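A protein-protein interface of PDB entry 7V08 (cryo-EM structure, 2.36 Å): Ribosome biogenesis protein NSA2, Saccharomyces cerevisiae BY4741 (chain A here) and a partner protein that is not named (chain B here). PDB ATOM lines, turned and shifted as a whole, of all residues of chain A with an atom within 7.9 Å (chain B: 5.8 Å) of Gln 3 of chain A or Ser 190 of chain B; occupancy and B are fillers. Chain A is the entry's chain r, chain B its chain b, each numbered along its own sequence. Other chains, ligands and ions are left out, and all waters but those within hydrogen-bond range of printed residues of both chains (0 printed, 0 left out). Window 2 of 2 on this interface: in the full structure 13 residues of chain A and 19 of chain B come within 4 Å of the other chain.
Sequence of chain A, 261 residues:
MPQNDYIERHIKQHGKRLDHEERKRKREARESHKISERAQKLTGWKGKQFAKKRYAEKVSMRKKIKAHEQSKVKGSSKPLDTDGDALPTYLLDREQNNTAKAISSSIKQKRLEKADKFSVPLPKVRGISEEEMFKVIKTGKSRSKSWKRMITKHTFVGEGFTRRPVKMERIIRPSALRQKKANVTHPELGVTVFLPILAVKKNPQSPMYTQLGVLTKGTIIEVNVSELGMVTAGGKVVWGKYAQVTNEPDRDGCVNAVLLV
The side-chain hydroxyl of Thr 188 of chain B sits at hydrogen-bond distance from the backbone NH of Ser 190 of chain B, at 3.1 Å. The side-chain hydroxyl of Ser 190 of chain B lies within hydrogen-bond range of the backbone carbonyl oxygen of Val 206 of chain B (3.3 Å). OD1 of Asp 5 of chain A lies within salt-bridge range of NH1 of Arg 9 of chain A (3.6 Å). NH1 of Arg 9 of chain A lies within hydrogen-bond range of O of Gln 3 of chain A, at 2.6 Å.
Of the 14 printed residues of chain B, 7 touch a printed residue of chain A. Among the printed residues, 12 pairs touch across the chains.
OG of Ser 190 of chain B sits at hydrogen-bond distance from NE2 of Gln 3 of chain A (3.1 Å). The side-chain carboxylate (OD2) of Asp 191 of chain B is in salt-bridge range of the guanidinium group (NH2) of Arg 9 of chain A (3.0 Å). O of Leu 204 of chain B is in hydrogen-bond range of ND2 of Asn 4 of chain A, 3.4 Å away. The backbone carbonyl oxygen (O) of Arg 159 of chain B is in hydrogen-bond range of the backbone NH (N) of Asn 4 of chain A (2.9 Å). The backbone carbonyl oxygen (O) of Val 206 of chain B is in hydrogen-bond range of the side-chain amide nitrogen (NE2) of Gln 3 of chain A (3.1 Å). The side-chain hydroxyl of Tyr 205 of chain B sits at hydrogen-bond distance from the guanidinium group of Arg 9 of chain A (3.4 Å).
Gln 3 of chain A touches Arg 159 of chain B. Gln 3 of chain A touches Pro 161 of chain B (OE1 to CB, 3.3 Å). Gln 3 of chain A touches Tyr 205 of chain B. Asn 4 of chain A touches Pro 161 of chain B (OD1 to CD, 3.7 Å). Tyr 205 of chain B touches Asn 4 of chain A (CZ to ND2, 3.2 Å). Arg 159 of chain B touches Tyr 6 of chain A.
Of the printed residues of chain B, Asn 4 of chain A touches Arg 159, Pro 161, Leu 204 and Tyr 205. Of chain A, only Gln 3 (3.1 Å) comes within 4 Å of Ser 190 of chain B. Printed residues of chain A within 4 Å of Asp 191 of chain B: Arg 9 (3.0 Å). Printed residues of chain A within 4 Å of Leu 204 of chain B: Asn 4 (3.4 Å). Of the printed residues of chain A, Tyr 205 of chain B touches Gln 3 (3.6 Å), Asn 4 (3.2 Å) and Arg 9 (3.4 Å). Printed residues of chain A within 4 Å of Val 206 of chain B: Gln 3. The nearest residue of chain A that does not touch Ser 190 of chain B is Arg 9 of chain A (6.6 Å).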
ATOM      1  N   PRO A   2     -13.064 -25.443  18.340  1.00  0.00           N
ATOM      2  CA  PRO A   2     -12.625 -26.096  19.569  1.00  0.00           C
ATOM      3  C   PRO A   2     -11.170 -26.553  19.441  1.00  0.00           C
ATOM      4  O   PRO A   2     -10.649 -26.623  18.336  1.00  0.00           O
ATOM      5  CB  PRO A   2     -13.595 -27.262  19.688  1.00  0.00           C
ATOM      6  CG  PRO A   2     -13.861 -27.640  18.267  1.00  0.00           C
ATOM      7  CD  PRO A   2     -13.747 -26.385  17.442  1.00  0.00           C
ATOM      8  N   GLN A   3     -10.507 -26.799  20.561  1.00  0.00           N
ATOM      9  CA  GLN A   3      -9.085 -27.088  20.561  1.00  0.00           C
ATOM     10  C   GLN A   3      -8.777 -28.134  21.619  1.00  0.00           C
ATOM     11  O   GLN A   3      -9.489 -28.253  22.619  1.00  0.00           O
ATOM     12  CB  GLN A   3      -8.261 -25.808  20.800  1.00  0.00           C
ATOM     13  CG  GLN A   3      -8.906 -24.821  21.759  1.00  0.00           C
ATOM     14  CD  GLN A   3      -8.137 -23.520  21.871  1.00  0.00           C
ATOM     15  OE1 GLN A   3      -6.972 -23.442  21.503  1.00  0.00           O
ATOM     16  NE2 GLN A   3      -8.789 -22.492  22.387  1.00  0.00           N
ATOM     17  N   ASN A   4      -7.729 -28.908  21.361  1.00  0.00           N
ATOM     18  CA  ASN A   4      -7.197 -29.931  22.276  1.00  0.00           C
ATOM     19  C   ASN A   4      -8.305 -30.955  22.547  1.00  0.00           C
ATOM     20  O   ASN A   4      -8.979 -31.394  21.605  1.00  0.00           O
ATOM     21  CB  ASN A   4      -6.606 -29.256  23.489  1.00  0.00           C
ATOM     22  CG  ASN A   4      -5.591 -28.194  23.116  1.00  0.00           C
ATOM     23  OD1 ASN A   4      -4.784 -28.382  22.211  1.00  0.00           O
ATOM     24  ND2 ASN A   4      -5.642 -27.067  23.797  1.00  0.00           N
ATOM     25  N   ASP A   5      -8.519 -31.368  23.793  1.00  0.00           N
ATOM     26  CA  ASP A   5      -9.432 -32.473  24.096  1.00  0.00           C
ATOM     27  C   ASP A   5     -10.817 -31.936  24.480  1.00  0.00           C
ATOM     28  O   ASP A   5     -11.312 -32.104  25.598  1.00  0.00           O
ATOM     29  CB  ASP A   5      -8.834 -33.355  25.185  1.00  0.00           C
ATOM     30  CG  ASP A   5      -8.462 -32.573  26.438  1.00  0.00           C
ATOM     31  OD1 ASP A   5      -8.394 -31.329  26.374  1.00  0.00           O
ATOM     32  OD2 ASP A   5      -8.245 -33.206  27.491  1.00  0.00           O
ATOM     33  N   TYR A   6     -11.461 -31.300  23.497  1.00  0.00           N
ATOM     34  CA  TYR A   6     -12.662 -30.527  23.791  1.00  0.00           C
ATOM     35  C   TYR A   6     -13.853 -31.407  24.162  1.00  0.00           C
ATOM     36  O   TYR A   6     -14.685 -30.984  24.963  1.00  0.00           O
ATOM     37  CB  TYR A   6     -13.007 -29.590  22.626  1.00  0.00           C
ATOM     38  CG  TYR A   6     -12.979 -30.187  21.240  1.00  0.00           C
ATOM     39  CD1 TYR A   6     -11.827 -30.141  20.468  1.00  0.00           C
ATOM     40  CD2 TYR A   6     -14.120 -30.752  20.684  1.00  0.00           C
ATOM     41  CE1 TYR A   6     -11.803 -30.667  19.199  1.00  0.00           C
ATOM     42  CE2 TYR A   6     -14.100 -31.285  19.416  1.00  0.00           C
ATOM     43  CZ  TYR A   6     -12.942 -31.244  18.681  1.00  0.00           C
ATOM     44  OH  TYR A   6     -12.932 -31.766  17.414  1.00  0.00           O
ATOM     45  N   ILE A   7     -13.950 -32.630  23.636  1.00  0.00           N
ATOM     46  CA  ILE A   7     -15.034 -33.524  24.041  1.00  0.00           C
ATOM     47  C   ILE A   7     -14.846 -33.987  25.484  1.00  0.00           C
ATOM     48  O   ILE A   7     -15.811 -34.055  26.254  1.00  0.00           O
ATOM     49  CB  ILE A   7     -15.159 -34.715  23.071  1.00  0.00           C
ATOM     50  CG1 ILE A   7     -15.588 -34.254  21.681  1.00  0.00           C
ATOM     51  CG2 ILE A   7     -16.161 -35.739  23.583  1.00  0.00           C
ATOM     52  CD1 ILE A   7     -16.868 -33.470  21.643  1.00  0.00           C
ATOM     53  N   ARG A   9     -13.230 -32.300  27.844  1.00  0.00           N
ATOM     54  CA  ARG A   9     -13.541 -31.124  28.653  1.00  0.00           C
ATOM     55  C   ARG A   9     -15.044 -30.865  28.703  1.00  0.00           C
ATOM     56  O   ARG A   9     -15.577 -30.468  29.743  1.00  0.00           O
ATOM     57  CB  ARG A   9     -12.809 -29.890  28.119  1.00  0.00           C
ATOM     58  CG  ARG A   9     -11.295 -30.025  28.027  1.00  0.00           C
ATOM     59  CD  ARG A   9     -10.609 -28.669  27.912  1.00  0.00           C
ATOM     60  NE  ARG A   9     -11.277 -27.777  26.971  1.00  0.00           N
ATOM     61  CZ  ARG A   9     -10.959 -27.657  25.690  1.00  0.00           C
ATOM     62  NH1 ARG A   9      -9.982 -28.364  25.149  1.00  0.00           N
ATOM     63  NH2 ARG A   9     -11.639 -26.805  24.932  1.00  0.00           N
ATOM     64  N   ARG B 159      -7.144 -31.779  16.066  1.00  0.00           N
ATOM     65  CA  ARG B 159      -7.670 -30.950  17.140  1.00  0.00           C
ATOM     66  C   ARG B 159      -6.690 -29.890  17.620  1.00  0.00           C
ATOM     67  O   ARG B 159      -6.975 -29.205  18.603  1.00  0.00           O
ATOM     68  CB  ARG B 159      -8.092 -31.820  18.321  1.00  0.00           C
ATOM     69  CG  ARG B 159      -9.140 -32.863  17.992  1.00  0.00           C
ATOM     70  CD  ARG B 159      -9.590 -33.569  19.244  1.00  0.00           C
ATOM     71  NE  ARG B 159      -8.464 -34.051  20.030  1.00  0.00           N
ATOM     72  CZ  ARG B 159      -8.057 -35.312  20.063  1.00  0.00           C
ATOM     73  NH1 ARG B 159      -8.687 -36.257  19.391  1.00  0.00           N
ATOM     74  NH2 ARG B 159      -6.993 -35.630  20.787  1.00  0.00           N
ATOM     75  N   LEU B 160      -5.548 -29.738  16.962  1.00  0.00           N
ATOM     76  CA  LEU B 160      -4.608 -28.698  17.356  1.00  0.00           C
ATOM     77  C   LEU B 160      -5.186 -27.321  17.040  1.00  0.00           C
ATOM     78  O   LEU B 160      -5.866 -27.156  16.024  1.00  0.00           O
ATOM     79  CB  LEU B 160      -3.272 -28.874  16.641  1.00  0.00           C
ATOM     80  CG  LEU B 160      -2.225 -29.797  17.261  1.00  0.00           C
ATOM     81  CD1 LEU B 160      -0.904 -29.616  16.531  1.00  0.00           C
ATOM     82  CD2 LEU B 160      -2.069 -29.540  18.754  1.00  0.00           C
ATOM     83  N   PRO B 161      -4.948 -26.325  17.892  1.00  0.00           N
ATOM     84  CA  PRO B 161      -5.386 -24.964  17.575  1.00  0.00           C
ATOM     85  C   PRO B 161      -4.627 -24.397  16.388  1.00  0.00           C
ATOM     86  O   PRO B 161      -3.462 -24.719  16.153  1.00  0.00           O
ATOM     87  CB  PRO B 161      -5.072 -24.183  18.853  1.00  0.00           C
ATOM     88  CG  PRO B 161      -3.942 -24.929  19.459  1.00  0.00           C
ATOM     89  CD  PRO B 161      -4.200 -26.378  19.157  1.00  0.00           C
ATOM     90  N   LEU B 184      -6.190 -15.158  30.170  1.00  0.00           N
ATOM     91  CA  LEU B 184      -6.692 -15.497  28.840  1.00  0.00           C
ATOM     92  C   LEU B 184      -8.213 -15.558  28.829  1.00  0.00           C
ATOM     93  O   LEU B 184      -8.855 -15.136  27.862  1.00  0.00           O
ATOM     94  CB  LEU B 184      -6.107 -16.823  28.363  1.00  0.00           C
ATOM     95  CG  LEU B 184      -6.532 -17.199  26.937  1.00  0.00           C
ATOM     96  CD1 LEU B 184      -5.753 -16.401  25.909  1.00  0.00           C
ATOM     97  CD2 LEU B 184      -6.409 -18.682  26.680  1.00  0.00           C
ATOM     98  N   ARG B 185      -8.802 -16.090  29.899  1.00  0.00           N
ATOM     99  CA  ARG B 185     -10.254 -16.113  30.020  1.00  0.00           C
ATOM    100  C   ARG B 185     -10.822 -14.705  30.118  1.00  0.00           C
ATOM    101  O   ARG B 185     -11.895 -14.423  29.576  1.00  0.00           O
ATOM    102  CB  ARG B 185     -10.660 -16.934  31.241  1.00  0.00           C
ATOM    103  CG  ARG B 185     -11.422 -18.193  30.922  1.00  0.00           C
ATOM    104  CD  ARG B 185     -12.100 -18.731  32.155  1.00  0.00           C
ATOM    105  NE  ARG B 185     -12.243 -20.179  32.103  1.00  0.00           N
ATOM    106  CZ  ARG B 185     -12.719 -20.914  33.095  1.00  0.00           C
ATOM    107  NH1 ARG B 185     -13.151 -20.363  34.216  1.00  0.00           N
ATOM    108  NH2 ARG B 185     -12.744 -22.237  32.967  1.00  0.00           N
ATOM    109  N   THR B 188     -10.173 -13.039  26.344  1.00  0.00           N
ATOM    110  CA  THR B 188     -10.783 -13.670  25.174  1.00  0.00           C
ATOM    111  C   THR B 188     -12.027 -14.445  25.584  1.00  0.00           C
ATOM    112  O   THR B 188     -12.477 -14.349  26.727  1.00  0.00           O
ATOM    113  CB  THR B 188      -9.804 -14.610  24.459  1.00  0.00           C
ATOM    114  OG1 THR B 188      -9.635 -15.808  25.226  1.00  0.00           O
ATOM    115  CG2 THR B 188      -8.452 -13.952  24.260  1.00  0.00           C
ATOM    116  N   LYS B 189     -12.599 -15.214  24.659  1.00  0.00           N
ATOM    117  CA  LYS B 189     -13.701 -16.106  24.989  1.00  0.00           C
ATOM    118  C   LYS B 189     -13.286 -17.569  24.887  1.00  0.00           C
ATOM    119  O   LYS B 189     -14.144 -18.452  24.830  1.00  0.00           O
ATOM    120  CB  LYS B 189     -14.927 -15.820  24.117  1.00  0.00           C
ATOM    121  CG  LYS B 189     -14.777 -16.146  22.652  1.00  0.00           C
ATOM    122  CD  LYS B 189     -16.141 -16.240  21.974  1.00  0.00           C
ATOM    123  CE  LYS B 189     -17.035 -15.056  22.315  1.00  0.00           C
ATOM    124  NZ  LYS B 189     -18.270 -15.063  21.494  1.00  0.00           N
ATOM    125  N   SER B 190     -11.983 -17.836  24.888  1.00  0.00           N
ATOM    126  CA  SER B 190     -11.484 -19.201  24.943  1.00  0.00           C
ATOM    127  C   SER B 190     -11.885 -19.862  26.257  1.00  0.00           C
ATOM    128  O   SER B 190     -12.003 -19.209  27.297  1.00  0.00           O
ATOM    129  CB  SER B 190      -9.964 -19.214  24.783  1.00  0.00           C
ATOM    130  OG  SER B 190      -9.470 -20.537  24.755  1.00  0.00           O
ATOM    131  N   ASP B 191     -12.094 -21.175  26.206  1.00  0.00           N
ATOM    132  CA  ASP B 191     -12.671 -21.926  27.322  1.00  0.00           C
ATOM    133  C   ASP B 191     -11.627 -22.710  28.107  1.00  0.00           C
ATOM    134  O   ASP B 191     -11.908 -23.812  28.584  1.00  0.00           O
ATOM    135  CB  ASP B 191     -13.763 -22.860  26.811  1.00  0.00           C
ATOM    136  CG  ASP B 191     -13.248 -23.852  25.784  1.00  0.00           C
ATOM    137  OD1 ASP B 191     -12.255 -23.541  25.097  1.00  0.00           O
ATOM    138  OD2 ASP B 191     -13.838 -24.942  25.656  1.00  0.00           O
ATOM    139  N   VAL B 192     -10.423 -22.159  28.266  1.00  0.00           N
ATOM    140  CA  VAL B 192      -9.361 -22.839  28.997  1.00  0.00           C
ATOM    141  C   VAL B 192      -9.739 -22.961  30.469  1.00  0.00           C
ATOM    142  O   VAL B 192     -10.218 -22.007  31.095  1.00  0.00           O
ATOM    143  CB  VAL B 192      -8.028 -22.093  28.808  1.00  0.00           C
ATOM    144  CG1 VAL B 192      -8.172 -20.627  29.186  1.00  0.00           C
ATOM    145  CG2 VAL B 192      -6.911 -22.758  29.606  1.00  0.00           C
ATOM    146  N   LEU B 204      -0.945 -25.724  24.253  1.00  0.00           N
ATOM    147  CA  LEU B 204      -1.159 -24.321  23.942  1.00  0.00           C
ATOM    148  C   LEU B 204      -2.630 -24.049  23.664  1.00  0.00           C
ATOM    149  O   LEU B 204      -3.280 -24.781  22.918  1.00  0.00           O
ATOM    150  CB  LEU B 204      -0.315 -23.912  22.740  1.00  0.00           C
ATOM    151  CG  LEU B 204       1.194 -23.957  22.954  1.00  0.00           C
ATOM    152  CD1 LEU B 204       1.916 -23.549  21.695  1.00  0.00           C
ATOM    153  CD2 LEU B 204       1.589 -23.058  24.113  1.00  0.00           C
ATOM    154  N   TYR B 205      -3.157 -22.992  24.276  1.00  0.00           N
ATOM    155  CA  TYR B 205      -4.518 -22.541  24.013  1.00  0.00           C
ATOM    156  C   TYR B 205      -4.465 -21.173  23.353  1.00  0.00           C
ATOM    157  O   TYR B 205      -3.579 -20.370  23.646  1.00  0.00           O
ATOM    158  CB  TYR B 205      -5.354 -22.486  25.299  1.00  0.00           C
ATOM    159  CG  TYR B 205      -5.883 -23.830  25.752  1.00  0.00           C
ATOM    160  CD1 TYR B 205      -5.072 -24.719  26.434  1.00  0.00           C
ATOM    161  CD2 TYR B 205      -7.198 -24.199  25.512  1.00  0.00           C
ATOM    162  CE1 TYR B 205      -5.536 -25.932  26.853  1.00  0.00           C
ATOM    163  CE2 TYR B 205      -7.680 -25.418  25.928  1.00  0.00           C
ATOM    164  CZ  TYR B 205      -6.842 -26.283  26.602  1.00  0.00           C
ATOM    165  OH  TYR B 205      -7.309 -27.505  27.018  1.00  0.00           O
ATOM    166  N   VAL B 206      -5.399 -20.918  22.444  1.00  0.00           N
ATOM    167  CA  VAL B 206      -5.434 -19.690  21.662  1.00  0.00           C
ATOM    168  C   VAL B 206      -6.757 -18.981  21.912  1.00  0.00           C
ATOM    169  O   VAL B 206      -7.805 -19.625  22.031  1.00  0.00           O
ATOM    170  CB  VAL B 206      -5.241 -19.969  20.156  1.00  0.00           C
ATOM    171  CG1 VAL B 206      -5.079 -18.674  19.381  1.00  0.00           C
ATOM    172  CG2 VAL B 206      -4.046 -20.856  19.936  1.00  0.00           C
ATOM    173  N   GLY B 207      -6.692 -17.653  22.038  1.00  0.00           N
ATOM    174  CA  GLY B 207      -7.873 -16.821  22.066  1.00  0.00           C
ATOM    175  C   GLY B 207      -7.694 -15.641  21.128  1.00  0.00           C
ATOM    176  O   GLY B 207      -6.611 -15.412  20.598  1.00  0.00           O
